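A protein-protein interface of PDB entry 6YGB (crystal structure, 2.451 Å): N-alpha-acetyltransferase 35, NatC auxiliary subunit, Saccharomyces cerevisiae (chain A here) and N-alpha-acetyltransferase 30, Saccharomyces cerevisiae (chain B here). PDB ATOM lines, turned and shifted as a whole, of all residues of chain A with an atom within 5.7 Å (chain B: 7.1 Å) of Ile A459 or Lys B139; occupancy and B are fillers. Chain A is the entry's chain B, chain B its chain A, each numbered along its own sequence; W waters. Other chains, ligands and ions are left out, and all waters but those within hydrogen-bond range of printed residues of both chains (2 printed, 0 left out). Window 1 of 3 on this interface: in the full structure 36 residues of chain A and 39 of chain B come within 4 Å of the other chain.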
ATOM      1  N   ARG A 410     -11.239  17.596  -9.244  1.00  0.00           N
ATOM      2  CA  ARG A 410     -11.305  16.168  -8.960  1.00  0.00           C
ATOM      3  C   ARG A 410     -10.042  15.692  -8.260  1.00  0.00           C
ATOM      4  O   ARG A 410     -10.115  14.913  -7.304  1.00  0.00           O
ATOM      5  CB  ARG A 410     -11.529  15.371 -10.241  1.00  0.00           C
ATOM      6  CG  ARG A 410     -11.540  13.881  -9.997  1.00  0.00           C
ATOM      7  CD  ARG A 410     -11.986  13.119 -11.217  1.00  0.00           C
ATOM      8  NE  ARG A 410     -12.318  11.737 -10.885  1.00  0.00           N
ATOM      9  CZ  ARG A 410     -11.440  10.741 -10.877  1.00  0.00           C
ATOM     10  NH1 ARG A 410     -10.169  10.978 -11.182  1.00  0.00           N
ATOM     11  NH2 ARG A 410     -11.834   9.512 -10.561  1.00  0.00           N
ATOM     12  N   GLN A 411      -8.877  16.155  -8.717  1.00  0.00           N
ATOM     13  CA  GLN A 411      -7.622  15.721  -8.112  1.00  0.00           C
ATOM     14  C   GLN A 411      -7.534  16.107  -6.643  1.00  0.00           C
ATOM     15  O   GLN A 411      -6.911  15.391  -5.854  1.00  0.00           O
ATOM     16  CB  GLN A 411      -6.447  16.306  -8.886  1.00  0.00           C
ATOM     17  CG  GLN A 411      -6.356  15.783 -10.296  1.00  0.00           C
ATOM     18  CD  GLN A 411      -5.556  16.687 -11.208  1.00  0.00           C
ATOM     19  OE1 GLN A 411      -4.651  17.395 -10.766  1.00  0.00           O
ATOM     20  NE2 GLN A 411      -5.891  16.670 -12.492  1.00  0.00           N
ATOM     21  N   GLY A 454     -15.463  12.025 -12.395  1.00  0.00           N
ATOM     22  CA  GLY A 454     -14.698  11.361 -13.437  1.00  0.00           C
ATOM     23  C   GLY A 454     -15.450  11.231 -14.750  1.00  0.00           C
ATOM     24  O   GLY A 454     -14.840  11.246 -15.821  1.00  0.00           O
ATOM     25  N   PHE A 455     -16.776  11.092 -14.693  1.00  0.00           N
ATOM     26  CA  PHE A 455     -17.563  11.019 -15.924  1.00  0.00           C
ATOM     27  C   PHE A 455     -17.561  12.357 -16.646  1.00  0.00           C
ATOM     28  O   PHE A 455     -17.494  12.405 -17.881  1.00  0.00           O
ATOM     29  CB  PHE A 455     -18.999  10.572 -15.627  1.00  0.00           C
ATOM     30  CG  PHE A 455     -19.136   9.097 -15.353  1.00  0.00           C
ATOM     31  CD1 PHE A 455     -18.972   8.164 -16.367  1.00  0.00           C
ATOM     32  CD2 PHE A 455     -19.454   8.648 -14.084  1.00  0.00           C
ATOM     33  CE1 PHE A 455     -19.111   6.809 -16.107  1.00  0.00           C
ATOM     34  CE2 PHE A 455     -19.592   7.301 -13.822  1.00  0.00           C
ATOM     35  CZ  PHE A 455     -19.418   6.381 -14.832  1.00  0.00           C
ATOM     36  N   ASP A 456     -17.615  13.455 -15.890  1.00  0.00           N
ATOM     37  CA  ASP A 456     -17.560  14.782 -16.493  1.00  0.00           C
ATOM     38  C   ASP A 456     -16.249  15.017 -17.227  1.00  0.00           C
ATOM     39  O   ASP A 456     -16.228  15.709 -18.250  1.00  0.00           O
ATOM     40  CB  ASP A 456     -17.765  15.852 -15.422  1.00  0.00           C
ATOM     41  CG  ASP A 456     -17.877  17.237 -16.008  1.00  0.00           C
ATOM     42  OD1 ASP A 456     -18.780  17.450 -16.846  1.00  0.00           O
ATOM     43  OD2 ASP A 456     -17.069  18.114 -15.635  1.00  0.00           O
ATOM     44  N   LEU A 457     -15.154  14.455 -16.729  1.00  0.00           N
ATOM     45  CA  LEU A 457     -13.851  14.618 -17.358  1.00  0.00           C
ATOM     46  C   LEU A 457     -13.537  13.514 -18.352  1.00  0.00           C
ATOM     47  O   LEU A 457     -12.405  13.454 -18.849  1.00  0.00           O
ATOM     48  CB  LEU A 457     -12.749  14.660 -16.304  1.00  0.00           C
ATOM     49  CG  LEU A 457     -12.881  15.755 -15.252  1.00  0.00           C
ATOM     50  CD1 LEU A 457     -11.869  15.544 -14.142  1.00  0.00           C
ATOM     51  CD2 LEU A 457     -12.705  17.120 -15.882  1.00  0.00           C
ATOM     52  N   ASP A 458     -14.509  12.642 -18.638  1.00  0.00           N
ATOM     53  CA  ASP A 458     -14.341  11.518 -19.564  1.00  0.00           C
ATOM     54  C   ASP A 458     -13.171  10.628 -19.158  1.00  0.00           C
ATOM     55  O   ASP A 458     -12.414  10.141 -20.000  1.00  0.00           O
ATOM     56  CB  ASP A 458     -14.182  12.000 -21.007  1.00  0.00           C
ATOM     57  CG  ASP A 458     -15.443  12.629 -21.548  1.00  0.00           C
ATOM     58  OD1 ASP A 458     -16.543  12.116 -21.246  1.00  0.00           O
ATOM     59  OD2 ASP A 458     -15.333  13.639 -22.273  1.00  0.00           O
ATOM     60  N   ILE A 459     -13.035  10.399 -17.853  1.00  0.00           N
ATOM     61  CA  ILE A 459     -11.942   9.574 -17.350  1.00  0.00           C
ATOM     62  C   ILE A 459     -12.249   8.099 -17.549  1.00  0.00           C
ATOM     63  O   ILE A 459     -11.358   7.298 -17.857  1.00  0.00           O
ATOM     64  CB  ILE A 459     -11.676   9.896 -15.869  1.00  0.00           C
ATOM     65  CG1 ILE A 459     -10.999  11.260 -15.739  1.00  0.00           C
ATOM     66  CG2 ILE A 459     -10.842   8.790 -15.214  1.00  0.00           C
ATOM     67  CD1 ILE A 459      -9.593  11.295 -16.292  1.00  0.00           C
ATOM     68  N   TYR A 460     -13.506   7.716 -17.369  1.00  0.00           N
ATOM     69  CA  TYR A 460     -13.913   6.325 -17.440  1.00  0.00           C
ATOM     70  C   TYR A 460     -14.329   5.967 -18.860  1.00  0.00           C
ATOM     71  O   TYR A 460     -15.041   6.727 -19.524  1.00  0.00           O
ATOM     72  CB  TYR A 460     -15.073   6.057 -16.481  1.00  0.00           C
ATOM     73  CG  TYR A 460     -14.935   6.677 -15.110  1.00  0.00           C
ATOM     74  CD1 TYR A 460     -13.825   6.427 -14.315  1.00  0.00           C
ATOM     75  CD2 TYR A 460     -15.941   7.482 -14.590  1.00  0.00           C
ATOM     76  CE1 TYR A 460     -13.711   6.980 -13.051  1.00  0.00           C
ATOM     77  CE2 TYR A 460     -15.836   8.036 -13.327  1.00  0.00           C
ATOM     78  CZ  TYR A 460     -14.719   7.784 -12.565  1.00  0.00           C
ATOM     79  OH  TYR A 460     -14.619   8.340 -11.313  1.00  0.00           O
ATOM     80  N   LYS A 461     -13.879   4.809 -19.319  1.00  0.00           N
ATOM     81  CA  LYS A 461     -14.285   4.314 -20.618  1.00  0.00           C
ATOM     82  C   LYS A 461     -15.658   3.654 -20.518  1.00  0.00           C
ATOM     83  O   LYS A 461     -16.101   3.287 -19.427  1.00  0.00           O
ATOM     84  CB  LYS A 461     -13.249   3.330 -21.154  1.00  0.00           C
ATOM     85  CG  LYS A 461     -11.948   3.981 -21.569  1.00  0.00           C
ATOM     86  CD  LYS A 461     -10.979   2.959 -22.137  1.00  0.00           C
ATOM     87  CE  LYS A 461     -11.471   2.398 -23.465  1.00  0.00           C
ATOM     88  NZ  LYS A 461     -11.629   3.457 -24.505  1.00  0.00           N
ATOM     89  N   GLU A 464     -16.188   0.619 -18.353  1.00  0.00           N
ATOM     90  CA  GLU A 464     -16.047   0.853 -16.922  1.00  0.00           C
ATOM     91  C   GLU A 464     -17.273   1.515 -16.313  1.00  0.00           C
ATOM     92  O   GLU A 464     -17.278   1.779 -15.108  1.00  0.00           O
ATOM     93  CB  GLU A 464     -14.820   1.730 -16.644  1.00  0.00           C
ATOM     94  CG  GLU A 464     -13.498   1.182 -17.167  1.00  0.00           C
ATOM     95  CD  GLU A 464     -12.313   2.079 -16.827  1.00  0.00           C
ATOM     96  OE1 GLU A 464     -12.176   3.157 -17.446  1.00  0.00           O
ATOM     97  OE2 GLU A 464     -11.522   1.711 -15.937  1.00  0.00           O
ATOM     98  N   ARG A 588      -8.288   1.036 -10.994  1.00  0.00           N
ATOM     99  CA  ARG A 588      -9.338   2.047 -11.090  1.00  0.00           C
ATOM    100  C   ARG A 588      -9.857   2.442  -9.712  1.00  0.00           C
ATOM    101  O   ARG A 588     -10.079   3.628  -9.444  1.00  0.00           O
ATOM    102  CB  ARG A 588     -10.474   1.535 -11.982  1.00  0.00           C
ATOM    103  CG  ARG A 588     -11.763   2.337 -11.900  1.00  0.00           C
ATOM    104  CD  ARG A 588     -11.584   3.767 -12.370  1.00  0.00           C
ATOM    105  NE  ARG A 588     -11.273   3.837 -13.794  1.00  0.00           N
ATOM    106  CZ  ARG A 588     -10.517   4.782 -14.347  1.00  0.00           C
ATOM    107  NH1 ARG A 588      -9.985   5.734 -13.593  1.00  0.00           N
ATOM    108  NH2 ARG A 588     -10.285   4.769 -15.654  1.00  0.00           N
ATOM    109  N   VAL B 121      -5.943  14.618 -25.032  1.00  0.00           N
ATOM    110  CA  VAL B 121      -7.307  14.110 -24.983  1.00  0.00           C
ATOM    111  C   VAL B 121      -7.920  14.044 -26.372  1.00  0.00           C
ATOM    112  O   VAL B 121      -8.867  13.280 -26.588  1.00  0.00           O
ATOM    113  CB  VAL B 121      -8.187  14.966 -24.053  1.00  0.00           C
ATOM    114  CG1 VAL B 121      -7.644  14.937 -22.625  1.00  0.00           C
ATOM    115  CG2 VAL B 121      -8.281  16.391 -24.566  1.00  0.00           C
ATOM    116  N   GLU B 131      -5.564   2.159 -25.014  1.00  0.00           N
ATOM    117  CA  GLU B 131      -6.681   1.605 -24.255  1.00  0.00           C
ATOM    118  C   GLU B 131      -7.057   0.213 -24.746  1.00  0.00           C
ATOM    119  O   GLU B 131      -7.498  -0.626 -23.955  1.00  0.00           O
ATOM    120  CB  GLU B 131      -7.874   2.555 -24.327  1.00  0.00           C
ATOM    121  CG  GLU B 131      -7.598   3.909 -23.684  1.00  0.00           C
ATOM    122  CD  GLU B 131      -8.580   4.983 -24.113  1.00  0.00           C
ATOM    123  OE1 GLU B 131      -9.507   4.672 -24.895  1.00  0.00           O
ATOM    124  OE2 GLU B 131      -8.421   6.140 -23.669  1.00  0.00           O
ATOM    125  N   ILE B 136      -5.809   2.430 -19.038  1.00  0.00           N
ATOM    126  CA  ILE B 136      -6.979   3.198 -18.638  1.00  0.00           C
ATOM    127  C   ILE B 136      -6.513   4.575 -18.195  1.00  0.00           C
ATOM    128  O   ILE B 136      -5.350   4.784 -17.849  1.00  0.00           O
ATOM    129  CB  ILE B 136      -7.804   2.518 -17.521  1.00  0.00           C
ATOM    130  CG1 ILE B 136      -6.936   2.255 -16.291  1.00  0.00           C
ATOM    131  CG2 ILE B 136      -8.468   1.249 -18.035  1.00  0.00           C
ATOM    132  CD1 ILE B 136      -7.686   1.622 -15.147  1.00  0.00           C
ATOM    133  N   ARG B 137      -7.442   5.519 -18.217  1.00  0.00           N
ATOM    134  CA  ARG B 137      -7.145   6.902 -17.877  1.00  0.00           C
ATOM    135  C   ARG B 137      -7.188   7.075 -16.362  1.00  0.00           C
ATOM    136  O   ARG B 137      -8.215   6.810 -15.731  1.00  0.00           O
ATOM    137  CB  ARG B 137      -8.147   7.826 -18.565  1.00  0.00           C
ATOM    138  CG  ARG B 137      -8.363   7.464 -20.021  1.00  0.00           C
ATOM    139  CD  ARG B 137      -9.410   8.328 -20.697  1.00  0.00           C
ATOM    140  NE  ARG B 137      -9.688   7.843 -22.045  1.00  0.00           N
ATOM    141  CZ  ARG B 137     -10.703   8.257 -22.796  1.00  0.00           C
ATOM    142  NH1 ARG B 137     -11.544   9.170 -22.333  1.00  0.00           N
ATOM    143  NH2 ARG B 137     -10.876   7.754 -24.008  1.00  0.00           N
ATOM    144  N   MET B 138      -6.076   7.511 -15.777  1.00  0.00           N
ATOM    145  CA  MET B 138      -6.003   7.708 -14.337  1.00  0.00           C
ATOM    146  C   MET B 138      -6.042   9.170 -13.930  1.00  0.00           C
ATOM    147  O   MET B 138      -6.149   9.459 -12.735  1.00  0.00           O
ATOM    148  CB  MET B 138      -4.735   7.058 -13.771  1.00  0.00           C
ATOM    149  CG  MET B 138      -4.719   5.553 -13.896  1.00  0.00           C
ATOM    150  SD  MET B 138      -6.220   4.803 -13.237  1.00  0.00           S
ATOM    151  CE  MET B 138      -6.092   5.247 -11.507  1.00  0.00           C
ATOM    152  N   LYS B 139      -5.984  10.091 -14.886  1.00  0.00           N
ATOM    153  CA  LYS B 139      -5.853  11.501 -14.558  1.00  0.00           C
ATOM    154  C   LYS B 139      -6.114  12.327 -15.811  1.00  0.00           C
ATOM    155  O   LYS B 139      -5.888  11.863 -16.933  1.00  0.00           O
ATOM    156  CB  LYS B 139      -4.456  11.786 -14.001  1.00  0.00           C
ATOM    157  CG  LYS B 139      -4.285  13.087 -13.262  1.00  0.00           C
ATOM    158  CD  LYS B 139      -2.888  13.124 -12.657  1.00  0.00           C
ATOM    159  CE  LYS B 139      -2.632  14.397 -11.887  1.00  0.00           C
ATOM    160  NZ  LYS B 139      -1.278  14.347 -11.277  1.00  0.00           N
ATOM    161  N   ARG B 140      -6.608  13.547 -15.608  1.00  0.00           N
ATOM    162  CA  ARG B 140      -6.760  14.525 -16.679  1.00  0.00           C
ATOM    163  C   ARG B 140      -6.077  15.806 -16.233  1.00  0.00           C
ATOM    164  O   ARG B 140      -6.344  16.298 -15.131  1.00  0.00           O
ATOM    165  CB  ARG B 140      -8.238  14.783 -17.014  1.00  0.00           C
ATOM    166  CG  ARG B 140      -8.460  15.680 -18.239  1.00  0.00           C
ATOM    167  CD  ARG B 140      -9.937  16.045 -18.416  1.00  0.00           C
ATOM    168  NE  ARG B 140     -10.187  16.860 -19.608  1.00  0.00           N
ATOM    169  CZ  ARG B 140     -10.804  16.417 -20.700  1.00  0.00           C
ATOM    170  NH1 ARG B 140     -11.244  15.167 -20.754  1.00  0.00           N
ATOM    171  NH2 ARG B 140     -10.992  17.220 -21.736  1.00  0.00           N
ATOM    172  N   MET B 141      -5.194  16.335 -17.079  1.00  0.00           N
ATOM    173  CA  MET B 141      -4.345  17.474 -16.742  1.00  0.00           C
ATOM    174  C   MET B 141      -4.795  18.694 -17.534  1.00  0.00           C
ATOM    175  O   MET B 141      -4.823  18.659 -18.767  1.00  0.00           O
ATOM    176  CB  MET B 141      -2.877  17.163 -17.034  1.00  0.00           C
ATOM    177  CG  MET B 141      -2.266  16.108 -16.129  1.00  0.00           C
ATOM    178  SD  MET B 141      -2.649  14.424 -16.645  1.00  0.00           S
ATOM    179  CE  MET B 141      -1.308  14.099 -17.782  1.00  0.00           C
ATOM    180  N   ALA B 151      -4.577  16.812 -21.242  1.00  0.00           N
ATOM    181  CA  ALA B 151      -3.921  15.527 -21.387  1.00  0.00           C
ATOM    182  C   ALA B 151      -4.650  14.483 -20.566  1.00  0.00           C
ATOM    183  O   ALA B 151      -5.336  14.806 -19.595  1.00  0.00           O
ATOM    184  CB  ALA B 151      -2.461  15.582 -20.934  1.00  0.00           C
ATOM    185  N   PHE B 152      -4.505  13.234 -20.983  1.00  0.00           N
ATOM    186  CA  PHE B 152      -4.854  12.089 -20.161  1.00  0.00           C
ATOM    187  C   PHE B 152      -3.566  11.416 -19.726  1.00  0.00           C
ATOM    188  O   PHE B 152      -2.607  11.333 -20.499  1.00  0.00           O
ATOM    189  CB  PHE B 152      -5.721  11.079 -20.915  1.00  0.00           C
ATOM    190  CG  PHE B 152      -7.165  11.458 -21.010  1.00  0.00           C
ATOM    191  CD1 PHE B 152      -7.844  11.949 -19.908  1.00  0.00           C
ATOM    192  CD2 PHE B 152      -7.847  11.314 -22.205  1.00  0.00           C
ATOM    193  CE1 PHE B 152      -9.178  12.294 -19.996  1.00  0.00           C
ATOM    194  CE2 PHE B 152      -9.184  11.657 -22.300  1.00  0.00           C
ATOM    195  CZ  PHE B 152      -9.848  12.150 -21.196  1.00  0.00           C
ATOM    196  N   LYS B 153      -3.545  10.958 -18.485  1.00  0.00           N
ATOM    197  CA  LYS B 153      -2.475  10.120 -17.976  1.00  0.00           C
ATOM    198  C   LYS B 153      -2.970   8.683 -18.043  1.00  0.00           C
ATOM    199  O   LYS B 153      -4.009   8.355 -17.458  1.00  0.00           O
ATOM    200  CB  LYS B 153      -2.112  10.516 -16.547  1.00  0.00           C
ATOM    201  CG  LYS B 153      -0.904   9.805 -15.955  1.00  0.00           C
ATOM    202  CD  LYS B 153      -0.598  10.359 -14.571  1.00  0.00           C
ATOM    203  CE  LYS B 153       0.745   9.878 -14.064  1.00  0.00           C
ATOM    204  NZ  LYS B 153       1.175  10.638 -12.860  1.00  0.00           N
ATOM    205  N   LEU B 154      -2.249   7.842 -18.779  1.00  0.00           N
ATOM    206  CA  LEU B 154      -2.630   6.454 -19.006  1.00  0.00           C
ATOM    207  C   LEU B 154      -1.667   5.531 -18.272  1.00  0.00           C
ATOM    208  O   LEU B 154      -0.445   5.711 -18.355  1.00  0.00           O
ATOM    209  CB  LEU B 154      -2.633   6.129 -20.503  1.00  0.00           C
ATOM    210  CG  LEU B 154      -3.499   7.022 -21.392  1.00  0.00           C
ATOM    211  CD1 LEU B 154      -3.451   6.589 -22.860  1.00  0.00           C
ATOM    212  CD2 LEU B 154      -4.922   7.027 -20.884  1.00  0.00           C
ATOM    213  N   ILE B 155      -2.215   4.538 -17.570  1.00  0.00           N
ATOM    214  CA  ILE B 155      -1.414   3.570 -16.832  1.00  0.00           C
ATOM    215  C   ILE B 155      -1.892   2.167 -17.168  1.00  0.00           C
ATOM    216  O   ILE B 155      -3.098   1.910 -17.231  1.00  0.00           O
ATOM    217  CB  ILE B 155      -1.462   3.833 -15.315  1.00  0.00           C
ATOM    218  CG1 ILE B 155      -0.626   5.067 -14.990  1.00  0.00           C
ATOM    219  CG2 ILE B 155      -0.921   2.639 -14.531  1.00  0.00           C
ATOM    220  CD1 ILE B 155      -1.188   5.904 -13.887  1.00  0.00           C
HETATM  221  O   HOH W   1     -10.215   5.182 -18.605  1.00  0.00           O
HETATM  222  O   HOH W   2      -8.233   8.075 -10.946  1.00  0.00           O
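The side-chain amino group (NZ) of Lys A461 lies within salt-bridge range of the side-chain carboxylate (OE1) of Glu B131 (2.5 Å). The backbone carbonyl oxygen (O) of Arg B137 is in hydrogen-bond range of the guanidinium group (NH2) of Arg A588 (2.9 Å). The side-chain amide nitrogen (NE2) of Gln A411 is in hydrogen-bond range of the backbone carbonyl oxygen (O) of Arg B140, 2.7 Å away. The backbone carbonyl oxygen of Asp A458 sits at hydrogen-bond distance from the guanidinium group of Arg B137 (2.7 Å). The backbone carbonyl oxygen of Leu A457 sits at hydrogen-bond distance from the guanidinium group of Arg B140 (2.8 Å).
The side-chain carboxylate (OE2) of Glu A464 is in salt-bridge range of the guanidinium group (NE) of Arg A588, at 3.0 Å. The backbone NH of Ile A459 lies within hydrogen-bond range of the backbone carbonyl oxygen of Gly A454, at 2.8 Å. The backbone NH (N) of Lys B153 lies within hydrogen-bond range of the backbone carbonyl oxygen (O) of Lys B139 (3.0 Å). The guanidinium group of Arg B137 is in salt-bridge range of the side-chain carboxylate of Glu B131. The side-chain carboxylate (OE1) of Glu A464 is in hydrogen-bond range of the backbone NH (N) of Lys A461 (3.0 Å). N of Met B138 lies within hydrogen-bond range of O of Lys B153 (2.8 Å).
Among the printed residues, merely in contact across the chains: Gln A411 with Lys B139 (3.8 Å), Leu A457 with Phe B152 (3.6 Å), Asp A458 with Phe B152 (3.5 Å), Ile A459 with Arg B137 (3.3 Å), Ile A459 with Lys B139 (3.7 Å), Ile A459 with Arg B140 (3.8 Å), Ile A459 with Phe B152 (3.9 Å), Glu A464 with Ile B136 (3.7 Å), Arg A588 with Ile B136 (3.8 Å) and Arg A588 with Met B138 (3.9 Å).
Gly A454 touches none of the printed residues of chain B. Phe A455 touches none of the printed residues of chain B. Of the printed residues of chain B, Asp A458 touches Arg B137 and Phe B152. Of chain B, only Arg B137 (3.3 Å), Lys B139 (3.7 Å), Arg B140 (3.8 Å) and Phe B152 (3.9 Å) come within 4 Å of Ile A459. Printed residues of chain A within 4 Å of Glu B131: Lys A461 (2.5 Å). Lys B139 touches two residues of chain A. The nearest residue of chain A that does not touch Lys B139 is Arg A410 (5.5 Å).
Of the 13 printed residues of chain B, 7 touch a printed residue of chain A. Printed residues of chain B that touch a printed residue of chain A: Glu B131, Ile B136, Arg B137, Met B138, Lys B139, Arg B140 and Phe B152. Hydrophobic or aromatic side chains of chain B that line the printed part of chain A: Ile B136, Met B138 and Phe B152. Of the 12 printed residues of chain A, 7 touch a printed residue of chain B.
Water W1 lies within hydrogen-bond range of the backbone carbonyl oxygen (O) of Ile A459 (2.5 Å), the backbone NH (N) of Arg B137 (2.8 Å), the guanidinium group (NH2) of Arg A588 (3.0 Å) and the side-chain carboxylate (OE1) of Glu A464 (3.0 Å). Water W2 lies within hydrogen-bond range of O of Met B138 (3.1 Å) and NH1 of Arg A410 (3.5 Å).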
